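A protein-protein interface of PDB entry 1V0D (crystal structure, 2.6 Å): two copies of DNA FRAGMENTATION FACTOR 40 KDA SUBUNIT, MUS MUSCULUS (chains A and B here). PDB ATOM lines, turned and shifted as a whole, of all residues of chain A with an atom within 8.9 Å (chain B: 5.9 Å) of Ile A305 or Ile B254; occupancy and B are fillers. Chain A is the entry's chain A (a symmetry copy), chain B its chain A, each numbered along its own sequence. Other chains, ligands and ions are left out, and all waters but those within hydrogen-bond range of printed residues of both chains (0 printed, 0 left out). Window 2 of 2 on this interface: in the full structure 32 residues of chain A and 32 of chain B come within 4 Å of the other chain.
Ile B254 touches one residue of chain A. Printed residues of chain B within 4 Å of His A242: Glu B251. Printed residues of chain A within 4 Å of Arg B250: Ala A306. Of the printed residues of chain B, His A304 touches Glu B251. Printed residues of chain A within 4 Å of Thr B258: Thr A258 and Ile A305. The nearest printed residue of chain B that does not touch Ile A305 is Leu B255 (4.01 Å).
Hydrophobic or aromatic side chains of chain B that line the printed part of chain A: Ile B254. Hydrophobic or aromatic side chains of chain A within 4 Å of the printed part of chain B: His A242, His A304, Ile A305 and Ala A306. Among the printed residues, 7 pairs touch across the chains. Among the printed residues, no Asp or Glu carboxylate lies within 4 Å of a Lys or Arg side-chain nitrogen of the other chain.
NH2 of Arg B250 lies within hydrogen-bond range of O of Ala A306 (3.3 Å). OE1 of Glu B251 sits at hydrogen-bond distance from NE2 of His A242 (2.7 Å).
CG2 of Thr B258 touches CG2 of Thr A258, at 3.4 Å. His A304 touches Glu B251. Ile B254 touches Ile A305 (CG2 to CG1, 3.8 Å). CD1 of Ile A305 touches CG2 of Thr B258 (3.9 Å). Glu B251 touches Ala A306.
The side-chain amide oxygen of Asn B249 is in hydrogen-bond range of the backbone NH of Glu B251, at 2.7 Å. The backbone carbonyl oxygen (O) of Ile B254 sits close to the side-chain hydroxyl (OG) of Ser B257 (2.9 Å). OG1 of Thr B258 is in hydrogen-bond range of O of Leu B255 (2.5 Å). The side-chain sulfur of Cys A229 lies close to the backbone NH of His A304. The backbone carbonyl oxygen (O) of Leu A255 lies within hydrogen-bond range of the side-chain hydroxyl (OG1) of Thr A258 (2.5 Å). N of Ala A306 is in hydrogen-bond range of ND1 of His A304 (2.7 Å).
Thr B258 touches its own counterpart, Thr A258. Positions printed for both chains: 255, 256, 257 and 258. Of the 7 pairs that touch across the chains among the printed residues, 1 has its exchanged pair printed and touching as well.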
ATOM      1  N   CYS A 229      17.006  14.037  16.715  1.00  0.00           N
ATOM      2  CA  CYS A 229      16.894  12.816  15.942  1.00  0.00           C
ATOM      3  C   CYS A 229      17.588  13.099  14.610  1.00  0.00           C
ATOM      4  O   CYS A 229      17.402  14.167  14.024  1.00  0.00           O
ATOM      5  CB  CYS A 229      15.423  12.476  15.703  1.00  0.00           C
ATOM      6  SG  CYS A 229      15.180  10.947  14.807  1.00  0.00           S
ATOM      7  N   PRO A 232      15.573   8.746   9.918  1.00  0.00           N
ATOM      8  CA  PRO A 232      15.945   7.368   9.587  1.00  0.00           C
ATOM      9  C   PRO A 232      17.266   7.261   8.814  1.00  0.00           C
ATOM     10  O   PRO A 232      17.791   8.258   8.312  1.00  0.00           O
ATOM     11  CB  PRO A 232      14.736   6.858   8.799  1.00  0.00           C
ATOM     12  CG  PRO A 232      14.125   8.101   8.249  1.00  0.00           C
ATOM     13  CD  PRO A 232      14.248   9.081   9.376  1.00  0.00           C
ATOM     14  N   CYS A 238      15.534  14.464  10.299  1.00  0.00           N
ATOM     15  CA  CYS A 238      14.275  14.023  10.904  1.00  0.00           C
ATOM     16  C   CYS A 238      13.132  14.935  10.500  1.00  0.00           C
ATOM     17  O   CYS A 238      13.064  16.091  10.913  1.00  0.00           O
ATOM     18  CB  CYS A 238      14.390  14.002  12.434  1.00  0.00           C
ATOM     19  SG  CYS A 238      12.838  13.638  13.321  1.00  0.00           S
ATOM     20  N   HIS A 242      12.349  15.428  15.957  1.00  0.00           N
ATOM     21  CA  HIS A 242      12.374  14.873  17.304  1.00  0.00           C
ATOM     22  C   HIS A 242      13.594  15.347  18.068  1.00  0.00           C
ATOM     23  O   HIS A 242      14.695  15.372  17.521  1.00  0.00           O
ATOM     24  CB  HIS A 242      12.456  13.353  17.238  1.00  0.00           C
ATOM     25  CG  HIS A 242      11.301  12.707  16.545  1.00  0.00           C
ATOM     26  ND1 HIS A 242      11.468  11.728  15.592  1.00  0.00           N
ATOM     27  CD2 HIS A 242       9.966  12.834  16.721  1.00  0.00           C
ATOM     28  CE1 HIS A 242      10.287  11.274  15.213  1.00  0.00           C
ATOM     29  NE2 HIS A 242       9.359  11.927  15.886  1.00  0.00           N
ATOM     30  N   ILE A 244      15.221  15.654  22.447  1.00  0.00           N
ATOM     31  CA  ILE A 244      15.028  15.121  23.782  1.00  0.00           C
ATOM     32  C   ILE A 244      16.194  15.523  24.660  1.00  0.00           C
ATOM     33  O   ILE A 244      17.341  15.523  24.209  1.00  0.00           O
ATOM     34  CB  ILE A 244      14.940  13.577  23.749  1.00  0.00           C
ATOM     35  CG1 ILE A 244      14.574  13.042  25.138  1.00  0.00           C
ATOM     36  CG2 ILE A 244      16.277  12.990  23.279  1.00  0.00           C
ATOM     37  CD1 ILE A 244      14.382  11.528  25.192  1.00  0.00           C
ATOM     38  N   LEU A 255      13.001   7.640  28.714  1.00  0.00           N
ATOM     39  CA  LEU A 255      12.561   7.636  27.326  1.00  0.00           C
ATOM     40  C   LEU A 255      13.780   7.543  26.408  1.00  0.00           C
ATOM     41  O   LEU A 255      13.734   6.918  25.348  1.00  0.00           O
ATOM     42  CB  LEU A 255      11.755   8.898  27.021  1.00  0.00           C
ATOM     43  CG  LEU A 255      10.341   8.901  27.613  1.00  0.00           C
ATOM     44  CD1 LEU A 255       9.748  10.282  27.505  1.00  0.00           C
ATOM     45  CD2 LEU A 255       9.470   7.891  26.883  1.00  0.00           C
ATOM     46  N   PHE A 256      14.882   8.149  26.831  1.00  0.00           N
ATOM     47  CA  PHE A 256      16.096   8.112  26.046  1.00  0.00           C
ATOM     48  C   PHE A 256      16.507   6.649  25.816  1.00  0.00           C
ATOM     49  O   PHE A 256      17.336   6.344  24.959  1.00  0.00           O
ATOM     50  CB  PHE A 256      17.189   8.891  26.779  1.00  0.00           C
ATOM     51  CG  PHE A 256      18.343   9.282  25.901  1.00  0.00           C
ATOM     52  CD1 PHE A 256      18.134  10.037  24.761  1.00  0.00           C
ATOM     53  CD2 PHE A 256      19.637   8.880  26.211  1.00  0.00           C
ATOM     54  CE1 PHE A 256      19.195  10.381  23.947  1.00  0.00           C
ATOM     55  CE2 PHE A 256      20.704   9.224  25.395  1.00  0.00           C
ATOM     56  CZ  PHE A 256      20.483   9.972  24.266  1.00  0.00           C
ATOM     57  N   SER A 257      15.922   5.742  26.588  1.00  0.00           N
ATOM     58  CA  SER A 257      16.213   4.316  26.434  1.00  0.00           C
ATOM     59  C   SER A 257      15.633   3.840  25.117  1.00  0.00           C
ATOM     60  O   SER A 257      16.145   2.898  24.509  1.00  0.00           O
ATOM     61  CB  SER A 257      15.567   3.496  27.548  1.00  0.00           C
ATOM     62  OG  SER A 257      16.154   3.802  28.791  1.00  0.00           O
ATOM     63  N   THR A 258      14.553   4.487  24.695  1.00  0.00           N
ATOM     64  CA  THR A 258      13.898   4.122  23.457  1.00  0.00           C
ATOM     65  C   THR A 258      14.597   4.705  22.237  1.00  0.00           C
ATOM     66  O   THR A 258      14.380   4.236  21.115  1.00  0.00           O
ATOM     67  CB  THR A 258      12.425   4.550  23.464  1.00  0.00           C
ATOM     68  OG1 THR A 258      12.335   5.976  23.542  1.00  0.00           O
ATOM     69  CG2 THR A 258      11.706   3.922  24.650  1.00  0.00           C
ATOM     70  N   TRP A 259      15.423   5.729  22.451  1.00  0.00           N
ATOM     71  CA  TRP A 259      16.182   6.325  21.354  1.00  0.00           C
ATOM     72  C   TRP A 259      17.300   5.349  21.059  1.00  0.00           C
ATOM     73  O   TRP A 259      18.002   4.907  21.963  1.00  0.00           O
ATOM     74  CB  TRP A 259      16.752   7.677  21.745  1.00  0.00           C
ATOM     75  CG  TRP A 259      15.735   8.741  21.638  1.00  0.00           C
ATOM     76  CD1 TRP A 259      14.556   8.817  22.321  1.00  0.00           C
ATOM     77  CD2 TRP A 259      15.794   9.904  20.805  1.00  0.00           C
ATOM     78  NE1 TRP A 259      13.874   9.960  21.968  1.00  0.00           N
ATOM     79  CE2 TRP A 259      14.613  10.647  21.040  1.00  0.00           C
ATOM     80  CE3 TRP A 259      16.733  10.395  19.884  1.00  0.00           C
ATOM     81  CZ2 TRP A 259      14.346  11.852  20.386  1.00  0.00           C
ATOM     82  CZ3 TRP A 259      16.467  11.592  19.238  1.00  0.00           C
ATOM     83  CH2 TRP A 259      15.281  12.308  19.492  1.00  0.00           C
ATOM     84  N   ASN A 260      17.469   5.026  19.787  1.00  0.00           N
ATOM     85  CA  ASN A 260      18.451   4.043  19.373  1.00  0.00           C
ATOM     86  C   ASN A 260      19.669   4.611  18.616  1.00  0.00           C
ATOM     87  O   ASN A 260      19.569   5.650  17.963  1.00  0.00           O
ATOM     88  CB  ASN A 260      17.685   3.030  18.516  1.00  0.00           C
ATOM     89  CG  ASN A 260      18.476   1.792  18.205  1.00  0.00           C
ATOM     90  OD1 ASN A 260      19.100   1.683  17.143  1.00  0.00           O
ATOM     91  ND2 ASN A 260      18.452   0.837  19.126  1.00  0.00           N
ATOM     92  N   LEU A 261      20.823   3.950  18.749  1.00  0.00           N
ATOM     93  CA  LEU A 261      22.038   4.315  18.001  1.00  0.00           C
ATOM     94  C   LEU A 261      22.021   3.293  16.853  1.00  0.00           C
ATOM     95  O   LEU A 261      22.602   2.210  16.955  1.00  0.00           O
ATOM     96  CB  LEU A 261      23.305   4.116  18.834  1.00  0.00           C
ATOM     97  CG  LEU A 261      23.752   5.221  19.790  1.00  0.00           C
ATOM     98  CD1 LEU A 261      25.147   4.898  20.319  1.00  0.00           C
ATOM     99  CD2 LEU A 261      23.770   6.547  19.082  1.00  0.00           C
ATOM    100  N   LEU A 302      21.721   8.580  15.552  1.00  0.00           N
ATOM    101  CA  LEU A 302      20.943   8.586  16.785  1.00  0.00           C
ATOM    102  C   LEU A 302      19.510   8.907  16.409  1.00  0.00           C
ATOM    103  O   LEU A 302      19.200  10.042  16.067  1.00  0.00           O
ATOM    104  CB  LEU A 302      21.462   9.648  17.753  1.00  0.00           C
ATOM    105  CG  LEU A 302      20.631   9.848  19.033  1.00  0.00           C
ATOM    106  CD1 LEU A 302      20.647   8.591  19.887  1.00  0.00           C
ATOM    107  CD2 LEU A 302      21.197  11.018  19.817  1.00  0.00           C
ATOM    108  N   VAL A 303      18.630   7.914  16.475  1.00  0.00           N
ATOM    109  CA  VAL A 303      17.235   8.135  16.104  1.00  0.00           C
ATOM    110  C   VAL A 303      16.208   7.872  17.189  1.00  0.00           C
ATOM    111  O   VAL A 303      16.376   7.001  18.050  1.00  0.00           O
ATOM    112  CB  VAL A 303      16.801   7.252  14.895  1.00  0.00           C
ATOM    113  CG1 VAL A 303      17.718   7.472  13.714  1.00  0.00           C
ATOM    114  CG2 VAL A 303      16.799   5.791  15.293  1.00  0.00           C
ATOM    115  N   HIS A 304      15.127   8.636  17.107  1.00  0.00           N
ATOM    116  CA  HIS A 304      13.978   8.506  17.985  1.00  0.00           C
ATOM    117  C   HIS A 304      13.367   7.199  17.486  1.00  0.00           C
ATOM    118  O   HIS A 304      13.611   6.800  16.355  1.00  0.00           O
ATOM    119  CB  HIS A 304      13.058   9.706  17.750  1.00  0.00           C
ATOM    120  CG  HIS A 304      11.680   9.566  18.317  1.00  0.00           C
ATOM    121  ND1 HIS A 304      10.740   8.705  17.786  1.00  0.00           N
ATOM    122  CD2 HIS A 304      11.047  10.265  19.288  1.00  0.00           C
ATOM    123  CE1 HIS A 304       9.584   8.890  18.397  1.00  0.00           C
ATOM    124  NE2 HIS A 304       9.743   9.830  19.313  1.00  0.00           N
ATOM    125  N   ILE A 305      12.593   6.522  18.314  1.00  0.00           N
ATOM    126  CA  ILE A 305      12.036   5.236  17.909  1.00  0.00           C
ATOM    127  C   ILE A 305      11.173   5.258  16.639  1.00  0.00           C
ATOM    128  O   ILE A 305      11.107   4.264  15.911  1.00  0.00           O
ATOM    129  CB  ILE A 305      11.238   4.598  19.076  1.00  0.00           C
ATOM    130  CG1 ILE A 305      10.812   3.183  18.689  1.00  0.00           C
ATOM    131  CG2 ILE A 305      10.044   5.479  19.447  1.00  0.00           C
ATOM    132  CD1 ILE A 305      10.096   2.451  19.776  1.00  0.00           C
ATOM    133  N   ALA A 306      10.528   6.386  16.365  1.00  0.00           N
ATOM    134  CA  ALA A 306       9.673   6.495  15.183  1.00  0.00           C
ATOM    135  C   ALA A 306      10.492   6.623  13.884  1.00  0.00           C
ATOM    136  O   ALA A 306       9.947   6.541  12.775  1.00  0.00           O
ATOM    137  CB  ALA A 306       8.727   7.694  15.331  1.00  0.00           C
ATOM    138  N   CYS A 307      11.795   6.833  14.035  1.00  0.00           N
ATOM    139  CA  CYS A 307      12.691   6.975  12.900  1.00  0.00           C
ATOM    140  C   CYS A 307      13.698   5.851  12.897  1.00  0.00           C
ATOM    141  O   CYS A 307      14.802   6.012  12.392  1.00  0.00           O
ATOM    142  CB  CYS A 307      13.440   8.311  12.952  1.00  0.00           C
ATOM    143  SG  CYS A 307      12.387   9.734  12.702  1.00  0.00           S
ATOM    144  N   HIS A 308      13.339   4.726  13.499  1.00  0.00           N
ATOM    145  CA  HIS A 308      14.225   3.577  13.504  1.00  0.00           C
ATOM    146  C   HIS A 308      13.562   2.557  12.611  1.00  0.00           C
ATOM    147  O   HIS A 308      12.740   1.773  13.074  1.00  0.00           O
ATOM    148  CB  HIS A 308      14.384   2.978  14.899  1.00  0.00           C
ATOM    149  CG  HIS A 308      15.389   1.866  14.965  1.00  0.00           C
ATOM    150  ND1 HIS A 308      15.535   1.057  16.070  1.00  0.00           N
ATOM    151  CD2 HIS A 308      16.333   1.462  14.081  1.00  0.00           C
ATOM    152  CE1 HIS A 308      16.525   0.206  15.867  1.00  0.00           C
ATOM    153  NE2 HIS A 308      17.028   0.430  14.668  1.00  0.00           N
ATOM    154  N   LYS A 309      13.884   2.587  11.327  1.00  0.00           N
ATOM    155  CA  LYS A 309      13.307   1.619  10.422  1.00  0.00           C
ATOM    156  C   LYS A 309      13.951   0.282  10.746  1.00  0.00           C
ATOM    157  O   LYS A 309      15.171   0.144  10.720  1.00  0.00           O
ATOM    158  CB  LYS A 309      13.569   2.017   8.969  1.00  0.00           C
ATOM    159  CG  LYS A 309      12.864   3.306   8.591  1.00  0.00           C
ATOM    160  CD  LYS A 309      13.038   3.675   7.122  1.00  0.00           C
ATOM    161  CE  LYS A 309      12.328   4.997   6.831  1.00  0.00           C
ATOM    162  NZ  LYS A 309      12.513   5.474   5.431  1.00  0.00           N
ATOM    163  N   LYS A 310      13.118  -0.691  11.094  1.00  0.00           N
ATOM    164  CA  LYS A 310      13.587  -2.022  11.436  1.00  0.00           C
ATOM    165  C   LYS A 310      13.634  -2.878  10.186  1.00  0.00           C
ATOM    166  O   LYS A 310      13.852  -4.087  10.255  1.00  0.00           O
ATOM    167  CB  LYS A 310      12.654  -2.656  12.469  1.00  0.00           C
ATOM    168  CG  LYS A 310      12.851  -2.143  13.891  1.00  0.00           C
ATOM    169  CD  LYS A 310      14.192  -2.601  14.449  1.00  0.00           C
ATOM    170  CE  LYS A 310      14.267  -2.380  15.959  1.00  0.00           C
ATOM    171  NZ  LYS A 310      15.538  -2.909  16.556  1.00  0.00           N
ATOM    172  N   ASN B 249      -2.541   8.027  15.384  1.00  0.00           N
ATOM    173  CA  ASN B 249      -1.297   8.627  14.944  1.00  0.00           C
ATOM    174  C   ASN B 249      -0.277   7.514  14.711  1.00  0.00           C
ATOM    175  O   ASN B 249      -0.238   6.534  15.456  1.00  0.00           O
ATOM    176  CB  ASN B 249      -0.859   9.557  16.073  1.00  0.00           C
ATOM    177  CG  ASN B 249       0.399  10.288  15.788  1.00  0.00           C
ATOM    178  OD1 ASN B 249       1.427   9.687  15.489  1.00  0.00           O
ATOM    179  ND2 ASN B 249       0.345  11.609  15.908  1.00  0.00           N
ATOM    180  N   ARG B 250       0.546   7.655  13.677  1.00  0.00           N
ATOM    181  CA  ARG B 250       1.558   6.651  13.372  1.00  0.00           C
ATOM    182  C   ARG B 250       2.585   6.568  14.491  1.00  0.00           C
ATOM    183  O   ARG B 250       2.903   5.489  14.978  1.00  0.00           O
ATOM    184  CB  ARG B 250       2.273   6.983  12.064  1.00  0.00           C
ATOM    185  CG  ARG B 250       3.478   6.112  11.838  1.00  0.00           C
ATOM    186  CD  ARG B 250       4.245   6.456  10.585  1.00  0.00           C
ATOM    187  NE  ARG B 250       5.438   5.618  10.515  1.00  0.00           N
ATOM    188  CZ  ARG B 250       6.639   5.978  10.962  1.00  0.00           C
ATOM    189  NH1 ARG B 250       6.829   7.184  11.501  1.00  0.00           N
ATOM    190  NH2 ARG B 250       7.641   5.106  10.918  1.00  0.00           N
ATOM    191  N   GLU B 251       3.111   7.717  14.891  1.00  0.00           N
ATOM    192  CA  GLU B 251       4.104   7.765  15.951  1.00  0.00           C
ATOM    193  C   GLU B 251       3.508   7.216  17.242  1.00  0.00           C
ATOM    194  O   GLU B 251       4.205   6.607  18.060  1.00  0.00           O
ATOM    195  CB  GLU B 251       4.562   9.202  16.158  1.00  0.00           C
ATOM    196  CG  GLU B 251       5.634   9.365  17.211  1.00  0.00           C
ATOM    197  CD  GLU B 251       6.286  10.734  17.151  1.00  0.00           C
ATOM    198  OE1 GLU B 251       6.825  11.084  16.070  1.00  0.00           O
ATOM    199  OE2 GLU B 251       6.259  11.453  18.178  1.00  0.00           O
ATOM    200  N   SER B 252       2.208   7.437  17.414  1.00  0.00           N
ATOM    201  CA  SER B 252       1.490   6.965  18.585  1.00  0.00           C
ATOM    202  C   SER B 252       1.444   5.437  18.574  1.00  0.00           C
ATOM    203  O   SER B 252       1.626   4.784  19.596  1.00  0.00           O
ATOM    204  CB  SER B 252       0.087   7.547  18.564  1.00  0.00           C
ATOM    205  OG  SER B 252      -0.657   7.124  19.684  1.00  0.00           O
ATOM    206  N   ARG B 253       1.214   4.869  17.402  1.00  0.00           N
ATOM    207  CA  ARG B 253       1.168   3.423  17.242  1.00  0.00           C
ATOM    208  C   ARG B 253       2.505   2.768  17.619  1.00  0.00           C
ATOM    209  O   ARG B 253       2.552   1.667  18.173  1.00  0.00           O
ATOM    210  CB  ARG B 253       0.842   3.100  15.787  1.00  0.00           C
ATOM    211  CG  ARG B 253       0.682   1.629  15.461  1.00  0.00           C
ATOM    212  CD  ARG B 253       0.895   1.414  13.975  1.00  0.00           C
ATOM    213  NE  ARG B 253       2.321   1.392  13.677  1.00  0.00           N
ATOM    214  CZ  ARG B 253       2.837   1.663  12.486  1.00  0.00           C
ATOM    215  NH1 ARG B 253       2.037   1.984  11.483  1.00  0.00           N
ATOM    216  NH2 ARG B 253       4.151   1.598  12.295  1.00  0.00           N
ATOM    217  N   ILE B 254       3.593   3.458  17.299  1.00  0.00           N
ATOM    218  CA  ILE B 254       4.948   2.976  17.563  1.00  0.00           C
ATOM    219  C   ILE B 254       5.358   3.131  19.027  1.00  0.00           C
ATOM    220  O   ILE B 254       6.040   2.262  19.582  1.00  0.00           O
ATOM    221  CB  ILE B 254       5.964   3.727  16.662  1.00  0.00           C
ATOM    222  CG1 ILE B 254       5.714   3.354  15.205  1.00  0.00           C
ATOM    223  CG2 ILE B 254       7.399   3.407  17.076  1.00  0.00           C
ATOM    224  CD1 ILE B 254       6.478   4.201  14.230  1.00  0.00           C
ATOM    225  N   LEU B 255       4.964   4.242  19.647  1.00  0.00           N
ATOM    226  CA  LEU B 255       5.297   4.466  21.046  1.00  0.00           C
ATOM    227  C   LEU B 255       4.645   3.382  21.904  1.00  0.00           C
ATOM    228  O   LEU B 255       5.204   2.942  22.908  1.00  0.00           O
ATOM    229  CB  LEU B 255       4.831   5.854  21.487  1.00  0.00           C
ATOM    230  CG  LEU B 255       5.689   7.006  20.955  1.00  0.00           C
ATOM    231  CD1 LEU B 255       4.988   8.317  21.201  1.00  0.00           C
ATOM    232  CD2 LEU B 255       7.050   6.997  21.632  1.00  0.00           C
ATOM    233  N   PHE B 256       3.467   2.935  21.489  1.00  0.00           N
ATOM    234  CA  PHE B 256       2.768   1.901  22.218  1.00  0.00           C
ATOM    235  C   PHE B 256       3.660   0.653  22.309  1.00  0.00           C
ATOM    236  O   PHE B 256       3.414  -0.255  23.104  1.00  0.00           O
ATOM    237  CB  PHE B 256       1.447   1.593  21.511  1.00  0.00           C
ATOM    238  CG  PHE B 256       0.457   0.864  22.370  1.00  0.00           C
ATOM    239  CD1 PHE B 256       0.044   1.401  23.577  1.00  0.00           C
ATOM    240  CD2 PHE B 256      -0.051  -0.368  21.976  1.00  0.00           C
ATOM    241  CE1 PHE B 256      -0.854   0.721  24.374  1.00  0.00           C
ATOM    242  CE2 PHE B 256      -0.954  -1.054  22.775  1.00  0.00           C
ATOM    243  CZ  PHE B 256      -1.354  -0.511  23.971  1.00  0.00           C
ATOM    244  N   SER B 257       4.702   0.610  21.488  1.00  0.00           N
ATOM    245  CA  SER B 257       5.638  -0.516  21.512  1.00  0.00           C
ATOM    246  C   SER B 257       6.424  -0.469  22.806  1.00  0.00           C
ATOM    247  O   SER B 257       6.862  -1.503  23.313  1.00  0.00           O
ATOM    248  CB  SER B 257       6.635  -0.429  20.361  1.00  0.00           C
ATOM    249  OG  SER B 257       5.980  -0.593  19.125  1.00  0.00           O
ATOM    250  N   THR B 258       6.612   0.740  23.325  1.00  0.00           N
ATOM    251  CA  THR B 258       7.355   0.921  24.552  1.00  0.00           C
ATOM    252  C   THR B 258       6.513   0.637  25.788  1.00  0.00           C
ATOM    253  O   THR B 258       7.059   0.421  26.875  1.00  0.00           O
ATOM    254  CB  THR B 258       7.943   2.335  24.641  1.00  0.00           C
ATOM    255  OG1 THR B 258       6.885   3.297  24.684  1.00  0.00           O
ATOM    256  CG2 THR B 258       8.835   2.603  23.435  1.00  0.00           C
